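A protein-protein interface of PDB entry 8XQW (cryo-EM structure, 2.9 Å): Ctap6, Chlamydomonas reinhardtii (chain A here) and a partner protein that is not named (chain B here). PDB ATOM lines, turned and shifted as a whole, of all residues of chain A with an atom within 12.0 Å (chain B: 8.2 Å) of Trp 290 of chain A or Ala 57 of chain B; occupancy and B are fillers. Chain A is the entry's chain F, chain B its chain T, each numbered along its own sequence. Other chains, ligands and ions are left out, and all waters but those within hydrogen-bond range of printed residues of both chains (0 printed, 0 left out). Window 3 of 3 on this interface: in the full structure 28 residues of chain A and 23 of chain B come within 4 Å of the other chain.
Of chain B, only Ala 57 and Pro 59 come within 4 Å of Trp 290 of chain A. Ala 57 of chain B touches just one residue of chain A: Trp 290. No residue of chain B comes within 4 Å of Ala 289 of chain A. Ala 55 of chain B touches none of the printed residues of chain A. No residue of chain A comes within 4 Å of Ala 56 of chain B. Pro 59 of chain B touches just these residues of chain A: Arg 287 (3.7 Å) and Trp 290 (3.3 Å). Of the printed residues of chain B, Leu 283 of chain A touches Pro 60 (3.97 Å). Of the printed residues of chain B, Glu 288 of chain A touches Gln 62. Printed residues of chain B within 4 Å of Arg 287 of chain A: Pro 59 (3.7 Å), Pro 60 (3.4 Å) and Gln 62 (2.7 Å). Printed residues of chain A within 4 Å of Pro 60 of chain B: Leu 283 and Arg 287. Of the printed residues of chain B, Leu 284 of chain A touches Gln 62 (3.98 Å). Ala 282 of chain A touches none of the printed residues of chain B. Ala 281 of chain A touches none of the printed residues of chain B. The nearest residue of chain B that does not touch Trp 290 of chain A is Leu 58 of chain B (4.1 Å).
Leu 283 of chain A touches Pro 60 of chain B (CD1 to CG, 3.97 Å). NE2 of Gln 62 of chain B touches CD2 of Leu 284 of chain A, 3.98 Å away. CG of Pro 59 of chain B touches NH2 of Arg 287 of chain A (3.7 Å). CD of Arg 287 of chain A touches O of Pro 60 of chain B, at 3.4 Å. Ala 57 of chain B touches Trp 290 of chain A (O to CZ3, 3.5 Å). Pro 59 of chain B touches Trp 290 of chain A.
The guanidinium group of Arg 287 of chain A is in hydrogen-bond range of the side-chain amide oxygen of Gln 62 of chain B (2.7 Å). The side-chain carboxylate of Glu 288 of chain A lies within hydrogen-bond range of the side-chain amide nitrogen of Gln 62 of chain B (3.4 Å).
Printed residues of chain A that touch a printed residue of chain B: Leu 283, Leu 284, Arg 287, Glu 288 and Trp 290. Hydrophobic or aromatic side chains of chain A that line the printed part of chain B: Leu 283, Leu 284 and Trp 290. Along chain A the printed residues that touch a printed residue of chain B span positions 283 to 290. Printed residues of chain B that touch a printed residue of chain A: Ala 57, Pro 59, Pro 60 and Gln 62. Among the printed residues, 8 pairs touch across the chains. Among the printed residues, no Asp or Glu carboxylate lies within 4 Å of a Lys or Arg side-chain nitrogen of the other chain.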
ATOM      1  N   ALA A 281       3.615 -14.654  12.295  1.00  0.00           N
ATOM      2  CA  ALA A 281       3.768 -15.805  13.173  1.00  0.00           C
ATOM      3  C   ALA A 281       4.139 -15.377  14.582  1.00  0.00           C
ATOM      4  O   ALA A 281       3.694 -15.991  15.551  1.00  0.00           O
ATOM      5  CB  ALA A 281       4.817 -16.760  12.607  1.00  0.00           C
ATOM      6  N   ALA A 282       4.947 -14.326  14.719  1.00  0.00           N
ATOM      7  CA  ALA A 282       5.235 -13.799  16.047  1.00  0.00           C
ATOM      8  C   ALA A 282       3.983 -13.214  16.678  1.00  0.00           C
ATOM      9  O   ALA A 282       3.725 -13.415  17.874  1.00  0.00           O
ATOM     10  CB  ALA A 282       6.338 -12.747  15.965  1.00  0.00           C
ATOM     11  N   LEU A 283       3.191 -12.490  15.883  1.00  0.00           N
ATOM     12  CA  LEU A 283       1.912 -11.997  16.382  1.00  0.00           C
ATOM     13  C   LEU A 283       1.069 -13.140  16.941  1.00  0.00           C
ATOM     14  O   LEU A 283       0.674 -13.128  18.120  1.00  0.00           O
ATOM     15  CB  LEU A 283       1.180 -11.263  15.255  1.00  0.00           C
ATOM     16  CG  LEU A 283      -0.113 -10.482  15.503  1.00  0.00           C
ATOM     17  CD1 LEU A 283      -1.324 -11.402  15.574  1.00  0.00           C
ATOM     18  CD2 LEU A 283       0.000  -9.628  16.760  1.00  0.00           C
ATOM     19  N   LEU A 284       0.824 -14.163  16.121  1.00  0.00           N
ATOM     20  CA  LEU A 284      -0.003 -15.279  16.562  1.00  0.00           C
ATOM     21  C   LEU A 284       0.624 -16.031  17.731  1.00  0.00           C
ATOM     22  O   LEU A 284      -0.097 -16.492  18.622  1.00  0.00           O
ATOM     23  CB  LEU A 284      -0.263 -16.223  15.393  1.00  0.00           C
ATOM     24  CG  LEU A 284      -1.693 -16.174  14.866  1.00  0.00           C
ATOM     25  CD1 LEU A 284      -1.815 -16.914  13.549  1.00  0.00           C
ATOM     26  CD2 LEU A 284      -2.621 -16.777  15.900  1.00  0.00           C
ATOM     27  N   ALA A 285       1.952 -16.164  17.752  1.00  0.00           N
ATOM     28  CA  ALA A 285       2.606 -16.933  18.800  1.00  0.00           C
ATOM     29  C   ALA A 285       2.466 -16.258  20.156  1.00  0.00           C
ATOM     30  O   ALA A 285       2.208 -16.925  21.168  1.00  0.00           O
ATOM     31  CB  ALA A 285       4.080 -17.139  18.451  1.00  0.00           C
ATOM     32  N   GLU A 286       2.641 -14.935  20.205  1.00  0.00           N
ATOM     33  CA  GLU A 286       2.430 -14.263  21.480  1.00  0.00           C
ATOM     34  C   GLU A 286       0.956 -14.277  21.855  1.00  0.00           C
ATOM     35  O   GLU A 286       0.624 -14.321  23.045  1.00  0.00           O
ATOM     36  CB  GLU A 286       2.970 -12.833  21.441  1.00  0.00           C
ATOM     37  CG  GLU A 286       3.895 -12.487  22.615  1.00  0.00           C
ATOM     38  CD  GLU A 286       3.175 -12.285  23.939  1.00  0.00           C
ATOM     39  OE1 GLU A 286       1.933 -12.173  23.949  1.00  0.00           O
ATOM     40  OE2 GLU A 286       3.861 -12.238  24.981  1.00  0.00           O
ATOM     41  N   ARG A 287       0.057 -14.270  20.864  1.00  0.00           N
ATOM     42  CA  ARG A 287      -1.358 -14.477  21.166  1.00  0.00           C
ATOM     43  C   ARG A 287      -1.569 -15.802  21.897  1.00  0.00           C
ATOM     44  O   ARG A 287      -2.225 -15.859  22.946  1.00  0.00           O
ATOM     45  CB  ARG A 287      -2.178 -14.432  19.875  1.00  0.00           C
ATOM     46  CG  ARG A 287      -3.348 -15.396  19.845  1.00  0.00           C
ATOM     47  CD  ARG A 287      -4.507 -14.847  20.649  1.00  0.00           C
ATOM     48  NE  ARG A 287      -5.527 -15.856  20.898  1.00  0.00           N
ATOM     49  CZ  ARG A 287      -6.671 -15.615  21.526  1.00  0.00           C
ATOM     50  NH1 ARG A 287      -7.545 -16.595  21.711  1.00  0.00           N
ATOM     51  NH2 ARG A 287      -6.944 -14.396  21.970  1.00  0.00           N
ATOM     52  N   GLU A 288      -1.004 -16.880  21.353  1.00  0.00           N
ATOM     53  CA  GLU A 288      -1.176 -18.191  21.962  1.00  0.00           C
ATOM     54  C   GLU A 288      -0.544 -18.268  23.342  1.00  0.00           C
ATOM     55  O   GLU A 288      -1.105 -18.918  24.232  1.00  0.00           O
ATOM     56  CB  GLU A 288      -0.598 -19.279  21.050  1.00  0.00           C
ATOM     57  CG  GLU A 288      -1.018 -19.192  19.574  1.00  0.00           C
ATOM     58  CD  GLU A 288      -2.529 -19.192  19.343  1.00  0.00           C
ATOM     59  OE1 GLU A 288      -2.941 -19.089  18.170  1.00  0.00           O
ATOM     60  OE2 GLU A 288      -3.310 -19.327  20.305  1.00  0.00           O
ATOM     61  N   ALA A 289       0.608 -17.618  23.540  1.00  0.00           N
ATOM     62  CA  ALA A 289       1.199 -17.553  24.873  1.00  0.00           C
ATOM     63  C   ALA A 289       0.281 -16.820  25.843  1.00  0.00           C
ATOM     64  O   ALA A 289       0.105 -17.252  26.988  1.00  0.00           O
ATOM     65  CB  ALA A 289       2.566 -16.877  24.811  1.00  0.00           C
ATOM     66  N   TRP A 290      -0.319 -15.711  25.394  1.00  0.00           N
ATOM     67  CA  TRP A 290      -1.359 -15.048  26.172  1.00  0.00           C
ATOM     68  C   TRP A 290      -2.461 -16.019  26.570  1.00  0.00           C
ATOM     69  O   TRP A 290      -2.976 -15.957  27.693  1.00  0.00           O
ATOM     70  CB  TRP A 290      -1.938 -13.867  25.383  1.00  0.00           C
ATOM     71  CG  TRP A 290      -3.439 -13.710  25.535  1.00  0.00           C
ATOM     72  CD1 TRP A 290      -4.408 -14.403  24.860  1.00  0.00           C
ATOM     73  CD2 TRP A 290      -4.133 -12.845  26.448  1.00  0.00           C
ATOM     74  NE1 TRP A 290      -5.654 -14.010  25.280  1.00  0.00           N
ATOM     75  CE2 TRP A 290      -5.514 -13.056  26.257  1.00  0.00           C
ATOM     76  CE3 TRP A 290      -3.720 -11.909  27.401  1.00  0.00           C
ATOM     77  CZ2 TRP A 290      -6.484 -12.361  26.981  1.00  0.00           C
ATOM     78  CZ3 TRP A 290      -4.682 -11.222  28.121  1.00  0.00           C
ATOM     79  CH2 TRP A 290      -6.048 -11.452  27.907  1.00  0.00           C
ATOM     80  N   VAL A 291      -2.853 -16.910  25.658  1.00  0.00           N
ATOM     81  CA  VAL A 291      -3.883 -17.889  26.003  1.00  0.00           C
ATOM     82  C   VAL A 291      -3.387 -18.816  27.106  1.00  0.00           C
ATOM     83  O   VAL A 291      -4.164 -19.268  27.957  1.00  0.00           O
ATOM     84  CB  VAL A 291      -4.327 -18.664  24.748  1.00  0.00           C
ATOM     85  CG1 VAL A 291      -5.489 -19.585  25.071  1.00  0.00           C
ATOM     86  CG2 VAL A 291      -4.751 -17.689  23.678  1.00  0.00           C
ATOM     87  N   ALA A 292      -2.089 -19.097  27.122  1.00  0.00           N
ATOM     88  CA  ALA A 292      -1.509 -19.908  28.183  1.00  0.00           C
ATOM     89  C   ALA A 292      -1.173 -19.033  29.382  1.00  0.00           C
ATOM     90  O   ALA A 292      -1.588 -17.876  29.453  1.00  0.00           O
ATOM     91  CB  ALA A 292      -0.272 -20.634  27.687  1.00  0.00           C
ATOM     92  N   VAL B  49     -10.785  -2.011  38.043  1.00  0.00           N
ATOM     93  CA  VAL B  49     -10.395  -1.828  36.652  1.00  0.00           C
ATOM     94  C   VAL B  49     -11.655  -1.638  35.825  1.00  0.00           C
ATOM     95  O   VAL B  49     -12.597  -2.430  35.930  1.00  0.00           O
ATOM     96  CB  VAL B  49      -9.575  -3.019  36.130  1.00  0.00           C
ATOM     97  CG1 VAL B  49      -8.952  -2.676  34.800  1.00  0.00           C
ATOM     98  CG2 VAL B  49      -8.503  -3.384  37.129  1.00  0.00           C
ATOM     99  N   PRO B  51     -14.345  -1.616  32.791  1.00  0.00           N
ATOM    100  CA  PRO B  51     -14.604  -2.541  31.679  1.00  0.00           C
ATOM    101  C   PRO B  51     -14.022  -2.055  30.369  1.00  0.00           C
ATOM    102  O   PRO B  51     -13.469  -2.861  29.613  1.00  0.00           O
ATOM    103  CB  PRO B  51     -16.136  -2.616  31.627  1.00  0.00           C
ATOM    104  CG  PRO B  51     -16.600  -2.107  32.953  1.00  0.00           C
ATOM    105  CD  PRO B  51     -15.588  -1.096  33.378  1.00  0.00           C
ATOM    106  N   ALA B  52     -14.129  -0.758  30.073  1.00  0.00           N
ATOM    107  CA  ALA B  52     -13.503  -0.228  28.868  1.00  0.00           C
ATOM    108  C   ALA B  52     -11.989  -0.179  29.018  1.00  0.00           C
ATOM    109  O   ALA B  52     -11.263  -0.040  28.026  1.00  0.00           O
ATOM    110  CB  ALA B  52     -14.062   1.157  28.548  1.00  0.00           C
ATOM    111  N   GLU B  53     -11.497  -0.278  30.255  1.00  0.00           N
ATOM    112  CA  GLU B  53     -10.074  -0.458  30.508  1.00  0.00           C
ATOM    113  C   GLU B  53      -9.636  -1.891  30.269  1.00  0.00           C
ATOM    114  O   GLU B  53      -8.603  -2.115  29.630  1.00  0.00           O
ATOM    115  CB  GLU B  53      -9.744  -0.066  31.949  1.00  0.00           C
ATOM    116  CG  GLU B  53      -8.288   0.275  32.216  1.00  0.00           C
ATOM    117  CD  GLU B  53      -8.107   1.116  33.471  1.00  0.00           C
ATOM    118  OE1 GLU B  53      -6.980   1.152  34.010  1.00  0.00           O
ATOM    119  OE2 GLU B  53      -9.090   1.737  33.926  1.00  0.00           O
ATOM    120  N   GLN B  54     -10.411  -2.858  30.764  1.00  0.00           N
ATOM    121  CA  GLN B  54     -10.055  -4.263  30.617  1.00  0.00           C
ATOM    122  C   GLN B  54     -10.211  -4.725  29.175  1.00  0.00           C
ATOM    123  O   GLN B  54      -9.445  -5.573  28.702  1.00  0.00           O
ATOM    124  CB  GLN B  54     -10.919  -5.111  31.548  1.00  0.00           C
ATOM    125  CG  GLN B  54     -10.562  -6.572  31.560  1.00  0.00           C
ATOM    126  CD  GLN B  54      -9.310  -6.848  32.358  1.00  0.00           C
ATOM    127  OE1 GLN B  54      -9.376  -7.206  33.535  1.00  0.00           O
ATOM    128  NE2 GLN B  54      -8.156  -6.682  31.724  1.00  0.00           N
ATOM    129  N   ALA B  55     -11.180  -4.163  28.456  1.00  0.00           N
ATOM    130  CA  ALA B  55     -11.467  -4.562  27.086  1.00  0.00           C
ATOM    131  C   ALA B  55     -10.333  -4.254  26.119  1.00  0.00           C
ATOM    132  O   ALA B  55     -10.455  -4.586  24.935  1.00  0.00           O
ATOM    133  CB  ALA B  55     -12.749  -3.884  26.608  1.00  0.00           C
ATOM    134  N   ALA B  56      -9.250  -3.629  26.574  1.00  0.00           N
ATOM    135  CA  ALA B  56      -8.122  -3.338  25.704  1.00  0.00           C
ATOM    136  C   ALA B  56      -6.958  -4.294  25.900  1.00  0.00           C
ATOM    137  O   ALA B  56      -6.125  -4.426  24.999  1.00  0.00           O
ATOM    138  CB  ALA B  56      -7.642  -1.900  25.925  1.00  0.00           C
ATOM    139  N   ALA B  57      -6.881  -4.964  27.046  1.00  0.00           N
ATOM    140  CA  ALA B  57      -5.768  -5.857  27.341  1.00  0.00           C
ATOM    141  C   ALA B  57      -5.808  -7.157  26.549  1.00  0.00           C
ATOM    142  O   ALA B  57      -4.904  -7.985  26.706  1.00  0.00           O
ATOM    143  CB  ALA B  57      -5.736  -6.168  28.838  1.00  0.00           C
ATOM    144  N   LEU B  58      -6.814  -7.358  25.704  1.00  0.00           N
ATOM    145  CA  LEU B  58      -6.900  -8.636  25.017  1.00  0.00           C
ATOM    146  C   LEU B  58      -6.391  -8.525  23.582  1.00  0.00           C
ATOM    147  O   LEU B  58      -6.619  -7.516  22.907  1.00  0.00           O
ATOM    148  CB  LEU B  58      -8.343  -9.150  25.026  1.00  0.00           C
ATOM    149  CG  LEU B  58      -9.393  -8.476  24.147  1.00  0.00           C
ATOM    150  CD1 LEU B  58      -9.696  -9.304  22.903  1.00  0.00           C
ATOM    151  CD2 LEU B  58     -10.658  -8.214  24.945  1.00  0.00           C
ATOM    152  N   PRO B  59      -5.695  -9.555  23.105  1.00  0.00           N
ATOM    153  CA  PRO B  59      -5.059  -9.487  21.792  1.00  0.00           C
ATOM    154  C   PRO B  59      -6.052  -9.822  20.698  1.00  0.00           C
ATOM    155  O   PRO B  59      -7.200 -10.188  20.990  1.00  0.00           O
ATOM    156  CB  PRO B  59      -3.962 -10.557  21.890  1.00  0.00           C
ATOM    157  CG  PRO B  59      -4.574 -11.598  22.750  1.00  0.00           C
ATOM    158  CD  PRO B  59      -5.469 -10.862  23.749  1.00  0.00           C
ATOM    159  N   PRO B  60      -5.661  -9.718  19.429  1.00  0.00           N
ATOM    160  CA  PRO B  60      -6.566 -10.138  18.357  1.00  0.00           C
ATOM    161  C   PRO B  60      -6.881 -11.620  18.465  1.00  0.00           C
ATOM    162  O   PRO B  60      -6.007 -12.451  18.731  1.00  0.00           O
ATOM    163  CB  PRO B  60      -5.783  -9.821  17.076  1.00  0.00           C
ATOM    164  CG  PRO B  60      -4.361  -9.724  17.509  1.00  0.00           C
ATOM    165  CD  PRO B  60      -4.414  -9.148  18.888  1.00  0.00           C
ATOM    166  N   SER B  61      -8.155 -11.941  18.267  1.00  0.00           N
ATOM    167  CA  SER B  61      -8.637 -13.306  18.400  1.00  0.00           C
ATOM    168  C   SER B  61      -8.443 -14.048  17.079  1.00  0.00           C
ATOM    169  O   SER B  61      -7.833 -13.539  16.135  1.00  0.00           O
ATOM    170  CB  SER B  61     -10.094 -13.311  18.860  1.00  0.00           C
ATOM    171  OG  SER B  61     -10.308 -12.371  19.899  1.00  0.00           O
ATOM    172  N   GLN B  62      -8.985 -15.264  17.000  1.00  0.00           N
ATOM    173  CA  GLN B  62      -8.609 -16.172  15.922  1.00  0.00           C
ATOM    174  C   GLN B  62      -9.195 -15.761  14.577  1.00  0.00           C
ATOM    175  O   GLN B  62      -8.666 -16.158  13.538  1.00  0.00           O
ATOM    176  CB  GLN B  62      -9.033 -17.597  16.271  1.00  0.00           C
ATOM    177  CG  GLN B  62      -8.494 -18.065  17.609  1.00  0.00           C
ATOM    178  CD  GLN B  62      -7.078 -17.581  17.864  1.00  0.00           C
ATOM    179  OE1 GLN B  62      -6.853 -16.672  18.664  1.00  0.00           O
ATOM    180  NE2 GLN B  62      -6.113 -18.189  17.182  1.00  0.00           N
